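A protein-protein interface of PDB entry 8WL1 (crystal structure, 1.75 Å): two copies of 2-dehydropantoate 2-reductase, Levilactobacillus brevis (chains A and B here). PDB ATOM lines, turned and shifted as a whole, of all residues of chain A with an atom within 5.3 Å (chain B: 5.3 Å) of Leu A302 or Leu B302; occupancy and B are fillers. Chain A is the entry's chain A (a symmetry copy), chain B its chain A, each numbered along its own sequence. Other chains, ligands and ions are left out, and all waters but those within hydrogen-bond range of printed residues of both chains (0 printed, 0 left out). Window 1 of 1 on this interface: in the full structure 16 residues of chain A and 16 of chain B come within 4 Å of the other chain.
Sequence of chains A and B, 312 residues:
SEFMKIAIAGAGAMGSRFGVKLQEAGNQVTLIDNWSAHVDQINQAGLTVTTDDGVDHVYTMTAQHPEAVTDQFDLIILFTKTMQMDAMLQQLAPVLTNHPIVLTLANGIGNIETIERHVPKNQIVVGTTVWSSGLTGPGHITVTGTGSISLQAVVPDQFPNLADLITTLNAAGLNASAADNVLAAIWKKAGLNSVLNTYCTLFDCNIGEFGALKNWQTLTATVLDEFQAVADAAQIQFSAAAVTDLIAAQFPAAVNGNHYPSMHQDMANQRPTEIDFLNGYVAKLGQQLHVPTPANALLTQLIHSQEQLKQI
The side-chain hydroxyl (OG) of Ser B305 is in hydrogen-bond range of the backbone carbonyl oxygen (O) of Gln B301 (3.2 Å).
O of Leu A219 sits at hydrogen-bond distance from OH of Tyr A199.
The side-chain hydroxyl (OG) of Ser A305 is in hydrogen-bond range of the backbone carbonyl oxygen (O) of Gln A301 (3.2 Å).
OH of Tyr B199 is in hydrogen-bond range of O of Leu B219 (2.8 Å).
Phe A203 touches Ser B305, and with the chains exchanged Ser A305 touches Phe B203.
Asn A215 touches Gln B301, and with the chains exchanged Gln A301 touches Asn B215.
Leu A219 touches Gln B301, and with the chains exchanged Gln A301 touches Leu B219.
Leu A302 touches its own counterpart, Leu B302.
Positions printed for both chains: 199, 202, 203, 215, 219, 298, 299, 300, 301, 302, 303, 304, 305, 306 and 307.
Of the 17 pairs that touch across the chains among the printed residues, 17 have their exchanged pair printed and touching as well.
Of the 15 printed residues of chain B, 8 touch a printed residue of chain A.
Hydrophobic or aromatic side chains of chain B that line the printed part of chain A: Tyr B199, Phe B203, Leu B219, Leu B298 and Leu B302.
Of the 15 printed residues of chain A, 8 touch a printed residue of chain B.
Among the printed residues, no Asp or Glu carboxylate lies within 4 Å of a Lys or Arg side-chain nitrogen of the other chain.
Of chain B, only Tyr B199, Phe B203 and Leu B302 come within 4 Å of Leu A302.
Of chain A, only Tyr A199, Phe A203 and Leu A302 come within 4 Å of Leu B302.
Printed residues of chain B within 4 Å of Asn A215: Gln B301 and Ser B305.
Printed residues of chain A within 4 Å of Ser B305: Phe A203, Asn A215 and Leu A219.
Leu A299 touches none of the printed residues of chain B.
Gln B306 touches none of the printed residues of chain A.
The side-chain amide oxygen (OD1) of Asn B215 lies within hydrogen-bond range of the side-chain hydroxyl (OG) of Ser A305, 2.8 Å away.
The side-chain amide nitrogen (ND2) of Asn B215 sits at hydrogen-bond distance from the side-chain amide oxygen (OE1) of Gln A301, 2.9 Å away.
The side-chain amide oxygen of Asn A215 lies within hydrogen-bond range of the side-chain hydroxyl of Ser B305 (2.8 Å).
OE1 of Gln B301 sits at hydrogen-bond distance from ND2 of Asn A215 (2.9 Å).
Among the printed residues, pairs that only touch across the chains: Tyr A199 with Leu B298, Tyr A199 with Leu B302, Phe A203 with Leu B302, Phe A203 with Ser B305, Leu A219 with Gln B301, Leu A219 with Ser B305, Leu A298 with Tyr B199, Gln A301 with Leu B219, Leu A302 with Tyr B199, Leu A302 with Phe B203, Leu A302 with Leu B302, Ser A305 with Phe B203 and Ser A305 with Leu B219.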
ATOM      1  N   TYR A 199       3.672 -16.632  27.077  1.00  0.00           N
ATOM      2  CA  TYR A 199       3.839 -15.205  27.233  1.00  0.00           C
ATOM      3  C   TYR A 199       5.112 -14.690  26.488  1.00  0.00           C
ATOM      4  O   TYR A 199       5.078 -13.629  25.882  1.00  0.00           O
ATOM      5  CB  TYR A 199       3.864 -14.820  28.699  1.00  0.00           C
ATOM      6  CG  TYR A 199       2.499 -14.841  29.391  1.00  0.00           C
ATOM      7  CD1 TYR A 199       1.432 -14.080  28.903  1.00  0.00           C
ATOM      8  CD2 TYR A 199       2.284 -15.577  30.546  1.00  0.00           C
ATOM      9  CE1 TYR A 199       0.218 -14.013  29.548  1.00  0.00           C
ATOM     10  CE2 TYR A 199       1.046 -15.549  31.176  1.00  0.00           C
ATOM     11  CZ  TYR A 199       0.007 -14.803  30.645  1.00  0.00           C
ATOM     12  OH  TYR A 199      -1.201 -14.706  31.240  1.00  0.00           O
ATOM     13  N   LEU A 202       4.116 -14.331  22.840  1.00  0.00           N
ATOM     14  CA  LEU A 202       3.245 -13.168  22.644  1.00  0.00           C
ATOM     15  C   LEU A 202       3.992 -11.883  22.730  1.00  0.00           C
ATOM     16  O   LEU A 202       3.743 -10.993  21.928  1.00  0.00           O
ATOM     17  CB  LEU A 202       2.107 -13.113  23.675  1.00  0.00           C
ATOM     18  CG  LEU A 202       1.015 -14.127  23.408  1.00  0.00           C
ATOM     19  CD1 LEU A 202       0.035 -14.178  24.596  1.00  0.00           C
ATOM     20  CD2 LEU A 202       0.299 -13.793  22.110  1.00  0.00           C
ATOM     21  N   PHE A 203       4.937 -11.793  23.671  1.00  0.00           N
ATOM     22  CA  PHE A 203       5.629 -10.539  23.910  1.00  0.00           C
ATOM     23  C   PHE A 203       6.925 -10.382  23.118  1.00  0.00           C
ATOM     24  O   PHE A 203       7.522  -9.324  23.182  1.00  0.00           O
ATOM     25  CB  PHE A 203       5.951 -10.372  25.385  1.00  0.00           C
ATOM     26  CG  PHE A 203       4.754 -10.311  26.309  1.00  0.00           C
ATOM     27  CD1 PHE A 203       3.559  -9.696  25.962  1.00  0.00           C
ATOM     28  CD2 PHE A 203       4.879 -10.826  27.609  1.00  0.00           C
ATOM     29  CE1 PHE A 203       2.510  -9.654  26.890  1.00  0.00           C
ATOM     30  CE2 PHE A 203       3.864 -10.763  28.543  1.00  0.00           C
ATOM     31  CZ  PHE A 203       2.652 -10.205  28.186  1.00  0.00           C
ATOM     32  N   ASN A 215       3.903  -6.808  36.112  1.00  0.00           N
ATOM     33  CA  ASN A 215       2.702  -7.635  36.300  1.00  0.00           C
ATOM     34  C   ASN A 215       2.950  -9.127  35.997  1.00  0.00           C
ATOM     35  O   ASN A 215       1.987  -9.862  35.699  1.00  0.00           O
ATOM     36  CB  ASN A 215       1.590  -7.065  35.448  1.00  0.00           C
ATOM     37  CG  ASN A 215       1.918  -7.129  33.973  1.00  0.00           C
ATOM     38  OD1 ASN A 215       3.077  -7.331  33.588  1.00  0.00           O
ATOM     39  ND2 ASN A 215       0.896  -6.965  33.136  1.00  0.00           N
ATOM     40  N   LEU A 219      -0.054 -12.120  35.488  1.00  0.00           N
ATOM     41  CA  LEU A 219      -0.143 -12.913  34.263  1.00  0.00           C
ATOM     42  C   LEU A 219      -0.007 -14.399  34.568  1.00  0.00           C
ATOM     43  O   LEU A 219      -0.725 -15.266  33.970  1.00  0.00           O
ATOM     44  CB  LEU A 219       0.954 -12.494  33.312  1.00  0.00           C
ATOM     45  CG  LEU A 219       0.835 -11.078  32.760  1.00  0.00           C
ATOM     46  CD1 LEU A 219       2.065 -10.855  31.888  1.00  0.00           C
ATOM     47  CD2 LEU A 219      -0.475 -10.868  31.997  1.00  0.00           C
ATOM     48  N   LEU A 298      -8.356 -17.790  25.444  1.00  0.00           N
ATOM     49  CA  LEU A 298      -7.948 -16.642  24.729  1.00  0.00           C
ATOM     50  C   LEU A 298      -6.456 -16.662  24.317  1.00  0.00           C
ATOM     51  O   LEU A 298      -6.104 -16.315  23.134  1.00  0.00           O
ATOM     52  CB  LEU A 298      -8.263 -15.357  25.538  1.00  0.00           C
ATOM     53  CG  LEU A 298      -7.879 -14.052  24.869  1.00  0.00           C
ATOM     54  CD1 LEU A 298      -8.506 -13.729  23.544  1.00  0.00           C
ATOM     55  CD2 LEU A 298      -8.211 -12.909  25.892  1.00  0.00           C
ATOM     56  N   LEU A 299      -5.573 -17.032  25.230  1.00  0.00           N
ATOM     57  CA  LEU A 299      -4.178 -17.082  24.924  1.00  0.00           C
ATOM     58  C   LEU A 299      -3.877 -17.989  23.725  1.00  0.00           C
ATOM     59  O   LEU A 299      -3.076 -17.647  22.853  1.00  0.00           O
ATOM     60  CB  LEU A 299      -3.337 -17.493  26.144  1.00  0.00           C
ATOM     61  CG  LEU A 299      -3.287 -16.434  27.281  1.00  0.00           C
ATOM     62  CD1 LEU A 299      -2.764 -17.035  28.575  1.00  0.00           C
ATOM     63  CD2 LEU A 299      -2.477 -15.207  26.882  1.00  0.00           C
ATOM     64  N   THR A 300      -4.579 -19.103  23.702  1.00  0.00           N
ATOM     65  CA  THR A 300      -4.491 -20.034  22.584  1.00  0.00           C
ATOM     66  C   THR A 300      -4.844 -19.362  21.253  1.00  0.00           C
ATOM     67  O   THR A 300      -4.124 -19.474  20.251  1.00  0.00           O
ATOM     68  CB  THR A 300      -5.322 -21.301  22.902  1.00  0.00           C
ATOM     69  OG1 THR A 300      -4.838 -21.949  24.082  1.00  0.00           O
ATOM     70  CG2 THR A 300      -5.261 -22.320  21.668  1.00  0.00           C
ATOM     71  N   GLN A 301      -5.955 -18.638  21.216  1.00  0.00           N
ATOM     72  CA  GLN A 301      -6.312 -17.871  20.045  1.00  0.00           C
ATOM     73  C   GLN A 301      -5.276 -16.847  19.662  1.00  0.00           C
ATOM     74  O   GLN A 301      -4.986 -16.686  18.472  1.00  0.00           O
ATOM     75  CB  GLN A 301      -7.686 -17.241  20.194  1.00  0.00           C
ATOM     76  CG  GLN A 301      -8.772 -18.275  20.399  1.00  0.00           C
ATOM     77  CD  GLN A 301      -8.914 -19.167  19.158  1.00  0.00           C
ATOM     78  OE1 GLN A 301      -8.760 -18.714  18.013  1.00  0.00           O
ATOM     79  NE2 GLN A 301      -9.172 -20.440  19.383  1.00  0.00           N
ATOM     80  N   LEU A 302      -4.726 -16.121  20.649  1.00  0.00           N
ATOM     81  CA  LEU A 302      -3.743 -15.092  20.327  1.00  0.00           C
ATOM     82  C   LEU A 302      -2.510 -15.696  19.641  1.00  0.00           C
ATOM     83  O   LEU A 302      -1.991 -15.151  18.670  1.00  0.00           O
ATOM     84  CB  LEU A 302      -3.338 -14.351  21.590  1.00  0.00           C
ATOM     85  CG  LEU A 302      -4.477 -13.637  22.347  1.00  0.00           C
ATOM     86  CD1 LEU A 302      -3.958 -12.970  23.595  1.00  0.00           C
ATOM     87  CD2 LEU A 302      -5.123 -12.603  21.477  1.00  0.00           C
ATOM     88  N   ILE A 303      -2.077 -16.849  20.124  1.00  0.00           N
ATOM     89  CA  ILE A 303      -0.904 -17.497  19.534  1.00  0.00           C
ATOM     90  C   ILE A 303      -1.185 -17.949  18.129  1.00  0.00           C
ATOM     91  O   ILE A 303      -0.362 -17.734  17.208  1.00  0.00           O
ATOM     92  CB  ILE A 303      -0.468 -18.703  20.401  1.00  0.00           C
ATOM     93  CG1 ILE A 303       0.169 -18.266  21.727  1.00  0.00           C
ATOM     94  CG2 ILE A 303       0.587 -19.534  19.684  1.00  0.00           C
ATOM     95  CD1 ILE A 303       1.455 -17.462  21.617  1.00  0.00           C
ATOM     96  N   HIS A 304      -2.344 -18.569  17.929  1.00  0.00           N
ATOM     97  CA  HIS A 304      -2.761 -18.897  16.548  1.00  0.00           C
ATOM     98  C   HIS A 304      -2.835 -17.713  15.589  1.00  0.00           C
ATOM     99  O   HIS A 304      -2.408 -17.831  14.426  1.00  0.00           O
ATOM    100  CB  HIS A 304      -4.041 -19.723  16.467  1.00  0.00           C
ATOM    101  CG  HIS A 304      -3.905 -21.112  16.996  1.00  0.00           C
ATOM    102  ND1 HIS A 304      -2.858 -21.950  16.649  1.00  0.00           N
ATOM    103  CD2 HIS A 304      -4.693 -21.822  17.835  1.00  0.00           C
ATOM    104  CE1 HIS A 304      -3.028 -23.108  17.259  1.00  0.00           C
ATOM    105  NE2 HIS A 304      -4.161 -23.076  17.934  1.00  0.00           N
ATOM    106  N   SER A 305      -3.338 -16.558  16.033  1.00  0.00           N
ATOM    107  CA  SER A 305      -3.313 -15.370  15.190  1.00  0.00           C
ATOM    108  C   SER A 305      -1.887 -14.947  14.849  1.00  0.00           C
ATOM    109  O   SER A 305      -1.574 -14.597  13.698  1.00  0.00           O
ATOM    110  CB  SER A 305      -4.024 -14.199  15.860  1.00  0.00           C
ATOM    111  OG  SER A 305      -5.370 -14.551  16.145  1.00  0.00           O
ATOM    112  N   GLN A 306      -1.032 -14.925  15.864  1.00  0.00           N
ATOM    113  CA  GLN A 306       0.371 -14.586  15.688  1.00  0.00           C
ATOM    114  C   GLN A 306       1.017 -15.489  14.622  1.00  0.00           C
ATOM    115  O   GLN A 306       1.805 -15.031  13.789  1.00  0.00           O
ATOM    116  CB  GLN A 306       1.086 -14.739  17.008  1.00  0.00           C
ATOM    117  CG  GLN A 306       2.389 -13.996  17.115  1.00  0.00           C
ATOM    118  CD  GLN A 306       3.034 -14.184  18.477  1.00  0.00           C
ATOM    119  OE1 GLN A 306       2.372 -14.619  19.445  1.00  0.00           O
ATOM    120  NE2 GLN A 306       4.340 -13.900  18.556  1.00  0.00           N
ATOM    121  N   GLU A 307       0.692 -16.770  14.674  1.00  0.00           N
ATOM    122  CA  GLU A 307       1.237 -17.726  13.690  1.00  0.00           C
ATOM    123  C   GLU A 307       0.850 -17.336  12.282  1.00  0.00           C
ATOM    124  O   GLU A 307       1.672 -17.390  11.339  1.00  0.00           O
ATOM    125  CB  GLU A 307       0.735 -19.123  13.934  1.00  0.00           C
ATOM    126  CG  GLU A 307       1.238 -19.821  15.173  1.00  0.00           C
ATOM    127  CD  GLU A 307       0.434 -21.079  15.514  1.00  0.00           C
ATOM    128  OE1 GLU A 307      -0.705 -21.266  15.019  1.00  0.00           O
ATOM    129  OE2 GLU A 307       0.918 -21.894  16.325  1.00  0.00           O
ATOM    130  N   TYR B 199      -6.227  -5.408  19.678  1.00  0.00           N
ATOM    131  CA  TYR B 199      -5.655  -6.538  18.983  1.00  0.00           C
ATOM    132  C   TYR B 199      -4.538  -6.095  17.984  1.00  0.00           C
ATOM    133  O   TYR B 199      -3.520  -6.761  17.871  1.00  0.00           O
ATOM    134  CB  TYR B 199      -6.732  -7.345  18.285  1.00  0.00           C
ATOM    135  CG  TYR B 199      -7.587  -8.213  19.212  1.00  0.00           C
ATOM    136  CD1 TYR B 199      -6.998  -9.166  20.050  1.00  0.00           C
ATOM    137  CD2 TYR B 199      -8.969  -8.117  19.223  1.00  0.00           C
ATOM    138  CE1 TYR B 199      -7.742 -10.018  20.833  1.00  0.00           C
ATOM    139  CE2 TYR B 199      -9.723  -8.944  20.047  1.00  0.00           C
ATOM    140  CZ  TYR B 199      -9.101  -9.857  20.881  1.00  0.00           C
ATOM    141  OH  TYR B 199      -9.787 -10.713  21.668  1.00  0.00           O
ATOM    142  N   LEU B 202      -1.404  -5.598  20.071  1.00  0.00           N
ATOM    143  CA  LEU B 202      -0.843  -6.885  20.493  1.00  0.00           C
ATOM    144  C   LEU B 202      -0.173  -7.602  19.373  1.00  0.00           C
ATOM    145  O   LEU B 202       0.894  -8.164  19.578  1.00  0.00           O
ATOM    146  CB  LEU B 202      -1.912  -7.824  21.073  1.00  0.00           C
ATOM    147  CG  LEU B 202      -2.359  -7.427  22.463  1.00  0.00           C
ATOM    148  CD1 LEU B 202      -3.586  -8.260  22.885  1.00  0.00           C
ATOM    149  CD2 LEU B 202      -1.213  -7.588  23.446  1.00  0.00           C
ATOM    150  N   PHE B 203      -0.771  -7.552  18.179  1.00  0.00           N
ATOM    151  CA  PHE B 203      -0.257  -8.323  17.061  1.00  0.00           C
ATOM    152  C   PHE B 203       0.734  -7.564  16.183  1.00  0.00           C
ATOM    153  O   PHE B 203       1.288  -8.160  15.279  1.00  0.00           O
ATOM    154  CB  PHE B 203      -1.391  -8.815  16.178  1.00  0.00           C
ATOM    155  CG  PHE B 203      -2.376  -9.751  16.846  1.00  0.00           C
ATOM    156  CD1 PHE B 203      -2.003 -10.696  17.792  1.00  0.00           C
ATOM    157  CD2 PHE B 203      -3.718  -9.724  16.434  1.00  0.00           C
ATOM    158  CE1 PHE B 203      -2.973 -11.547  18.338  1.00  0.00           C
ATOM    159  CE2 PHE B 203      -4.677 -10.578  16.941  1.00  0.00           C
ATOM    160  CZ  PHE B 203      -4.325 -11.480  17.925  1.00  0.00           C
ATOM    161  N   ASN B 215      -9.323 -16.379  12.733  1.00  0.00           N
ATOM    162  CA  ASN B 215     -10.094 -16.343  13.984  1.00  0.00           C
ATOM    163  C   ASN B 215     -10.494 -14.912  14.399  1.00  0.00           C
ATOM    164  O   ASN B 215     -10.759 -14.669  15.593  1.00  0.00           O
ATOM    165  CB  ASN B 215      -9.291 -17.036  15.062  1.00  0.00           C
ATOM    166  CG  ASN B 215      -7.990 -16.319  15.348  1.00  0.00           C
ATOM    167  OD1 ASN B 215      -7.544 -15.474  14.563  1.00  0.00           O
ATOM    168  ND2 ASN B 215      -7.376 -16.647  16.484  1.00  0.00           N
ATOM    169  N   LEU B 219     -12.016 -13.733  18.211  1.00  0.00           N
ATOM    170  CA  LEU B 219     -11.351 -12.709  19.016  1.00  0.00           C
ATOM    171  C   LEU B 219     -12.293 -11.546  19.298  1.00  0.00           C
ATOM    172  O   LEU B 219     -12.319 -10.977  20.439  1.00  0.00           O
ATOM    173  CB  LEU B 219     -10.135 -12.201  18.278  1.00  0.00           C
ATOM    174  CG  LEU B 219      -9.011 -13.214  18.096  1.00  0.00           C
ATOM    175  CD1 LEU B 219      -7.930 -12.511  17.282  1.00  0.00           C
ATOM    176  CD2 LEU B 219      -8.491 -13.741  19.436  1.00  0.00           C
ATOM    177  N   LEU B 298      -7.547  -9.599  31.051  1.00  0.00           N
ATOM    178  CA  LEU B 298      -6.313 -10.089  30.569  1.00  0.00           C
ATOM    179  C   LEU B 298      -5.696  -9.224  29.442  1.00  0.00           C
ATOM    180  O   LEU B 298      -4.449  -8.929  29.457  1.00  0.00           O
ATOM    181  CB  LEU B 298      -6.459 -11.558  30.096  1.00  0.00           C
ATOM    182  CG  LEU B 298      -5.196 -12.203  29.562  1.00  0.00           C
ATOM    183  CD1 LEU B 298      -4.014 -12.304  30.482  1.00  0.00           C
ATOM    184  CD2 LEU B 298      -5.595 -13.640  29.074  1.00  0.00           C
ATOM    185  N   LEU B 299      -6.499  -8.822  28.470  1.00  0.00           N
ATOM    186  CA  LEU B 299      -6.006  -8.015  27.399  1.00  0.00           C
ATOM    187  C   LEU B 299      -5.347  -6.723  27.897  1.00  0.00           C
ATOM    188  O   LEU B 299      -4.289  -6.320  27.412  1.00  0.00           O
ATOM    189  CB  LEU B 299      -7.100  -7.705  26.363  1.00  0.00           C
ATOM    190  CG  LEU B 299      -7.570  -8.932  25.532  1.00  0.00           C
ATOM    191  CD1 LEU B 299      -8.875  -8.645  24.809  1.00  0.00           C
ATOM    192  CD2 LEU B 299      -6.498  -9.406  24.558  1.00  0.00           C
ATOM    193  N   THR B 300      -5.982  -6.145  28.896  1.00  0.00           N
ATOM    194  CA  THR B 300      -5.444  -4.963  29.556  1.00  0.00           C
ATOM    195  C   THR B 300      -4.042  -5.214  30.122  1.00  0.00           C
ATOM    196  O   THR B 300      -3.101  -4.437  29.911  1.00  0.00           O
ATOM    197  CB  THR B 300      -6.468  -4.439  30.592  1.00  0.00           C
ATOM    198  OG1 THR B 300      -7.704  -4.093  29.961  1.00  0.00           O
ATOM    199  CG2 THR B 300      -5.876  -3.158  31.349  1.00  0.00           C
ATOM    200  N   GLN B 301      -3.868  -6.314  30.843  1.00  0.00           N
ATOM    201  CA  GLN B 301      -2.560  -6.700  31.320  1.00  0.00           C
ATOM    202  C   GLN B 301      -1.558  -6.907  30.216  1.00  0.00           C
ATOM    203  O   GLN B 301      -0.404  -6.489  30.351  1.00  0.00           O
ATOM    204  CB  GLN B 301      -2.640  -7.913  32.232  1.00  0.00           C
ATOM    205  CG  GLN B 301      -3.503  -7.660  33.449  1.00  0.00           C
ATOM    206  CD  GLN B 301      -2.881  -6.575  34.340  1.00  0.00           C
ATOM    207  OE1 GLN B 301      -1.652  -6.474  34.476  1.00  0.00           O
ATOM    208  NE2 GLN B 301      -3.724  -5.744  34.919  1.00  0.00           N
ATOM    209  N   LEU B 302      -1.965  -7.575  29.125  1.00  0.00           N
ATOM    210  CA  LEU B 302      -1.022  -7.833  28.041  1.00  0.00           C
ATOM    211  C   LEU B 302      -0.494  -6.523  27.441  1.00  0.00           C
ATOM    212  O   LEU B 302       0.695  -6.384  27.166  1.00  0.00           O
ATOM    213  CB  LEU B 302      -1.687  -8.679  26.967  1.00  0.00           C
ATOM    214  CG  LEU B 302      -2.208 -10.057  27.422  1.00  0.00           C
ATOM    215  CD1 LEU B 302      -2.874 -10.784  26.281  1.00  0.00           C
ATOM    216  CD2 LEU B 302      -1.086 -10.900  27.944  1.00  0.00           C
ATOM    217  N   ILE B 303      -1.378  -5.551  27.287  1.00  0.00           N
ATOM    218  CA  ILE B 303      -0.964  -4.267  26.719  1.00  0.00           C
ATOM    219  C   ILE B 303      -0.018  -3.548  27.638  1.00  0.00           C
ATOM    220  O   ILE B 303       1.027  -3.014  27.197  1.00  0.00           O
ATOM    221  CB  ILE B 303      -2.202  -3.382  26.438  1.00  0.00           C
ATOM    222  CG1 ILE B 303      -3.024  -3.893  25.246  1.00  0.00           C
ATOM    223  CG2 ILE B 303      -1.787  -1.962  26.082  1.00  0.00           C
ATOM    224  CD1 ILE B 303      -2.315  -3.898  23.901  1.00  0.00           C
ATOM    225  N   HIS B 304      -0.348  -3.526  28.926  1.00  0.00           N
ATOM    226  CA  HIS B 304       0.612  -2.980  29.911  1.00  0.00           C
ATOM    227  C   HIS B 304       1.985  -3.643  29.922  1.00  0.00           C
ATOM    228  O   HIS B 304       3.009  -2.943  30.025  1.00  0.00           O
ATOM    229  CB  HIS B 304       0.058  -2.888  31.329  1.00  0.00           C
ATOM    230  CG  HIS B 304      -1.031  -1.881  31.496  1.00  0.00           C
ATOM    231  ND1 HIS B 304      -0.939  -0.587  31.012  1.00  0.00           N
ATOM    232  CD2 HIS B 304      -2.232  -1.969  32.109  1.00  0.00           C
ATOM    233  CE1 HIS B 304      -2.043   0.060  31.332  1.00  0.00           C
ATOM    234  NE2 HIS B 304      -2.815  -0.734  32.047  1.00  0.00           N
ATOM    235  N   SER B 305       2.059  -4.970  29.791  1.00  0.00           N
ATOM    236  CA  SER B 305       3.351  -5.630  29.672  1.00  0.00           C
ATOM    237  C   SER B 305       4.104  -5.179  28.423  1.00  0.00           C
ATOM    238  O   SER B 305       5.319  -4.917  28.459  1.00  0.00           O
ATOM    239  CB  SER B 305       3.200  -7.147  29.632  1.00  0.00           C
ATOM    240  OG  SER B 305       2.544  -7.597  30.808  1.00  0.00           O
ATOM    241  N   GLN B 306       3.395  -5.143  27.302  1.00  0.00           N
ATOM    242  CA  GLN B 306       3.961  -4.693  26.041  1.00  0.00           C
ATOM    243  C   GLN B 306       4.570  -3.288  26.191  1.00  0.00           C
ATOM    244  O   GLN B 306       5.647  -2.998  25.663  1.00  0.00           O
ATOM    245  CB  GLN B 306       2.881  -4.686  24.988  1.00  0.00           C
ATOM    246  CG  GLN B 306       3.376  -4.708  23.568  1.00  0.00           C
ATOM    247  CD  GLN B 306       2.230  -4.722  22.572  1.00  0.00           C
ATOM    248  OE1 GLN B 306       1.070  -5.017  22.933  1.00  0.00           O
ATOM    249  NE2 GLN B 306       2.533  -4.361  21.319  1.00  0.00           N
ATOM    250  N   GLU B 307       3.859  -2.421  26.895  1.00  0.00           N
ATOM    251  CA  GLU B 307       4.354  -1.049  27.120  1.00  0.00           C
ATOM    252  C   GLU B 307       5.682  -1.062  27.841  1.00  0.00           C
ATOM    253  O   GLU B 307       6.618  -0.302  27.502  1.00  0.00           O
ATOM    254  CB  GLU B 307       3.391  -0.238  27.945  1.00  0.00           C
ATOM    255  CG  GLU B 307       2.084   0.138  27.293  1.00  0.00           C
ATOM    256  CD  GLU B 307       1.048   0.658  28.294  1.00  0.00           C
ATOM    257  OE1 GLU B 307       1.180   0.441  29.524  1.00  0.00           O
ATOM    258  OE2 GLU B 307       0.052   1.267  27.858  1.00  0.00           O
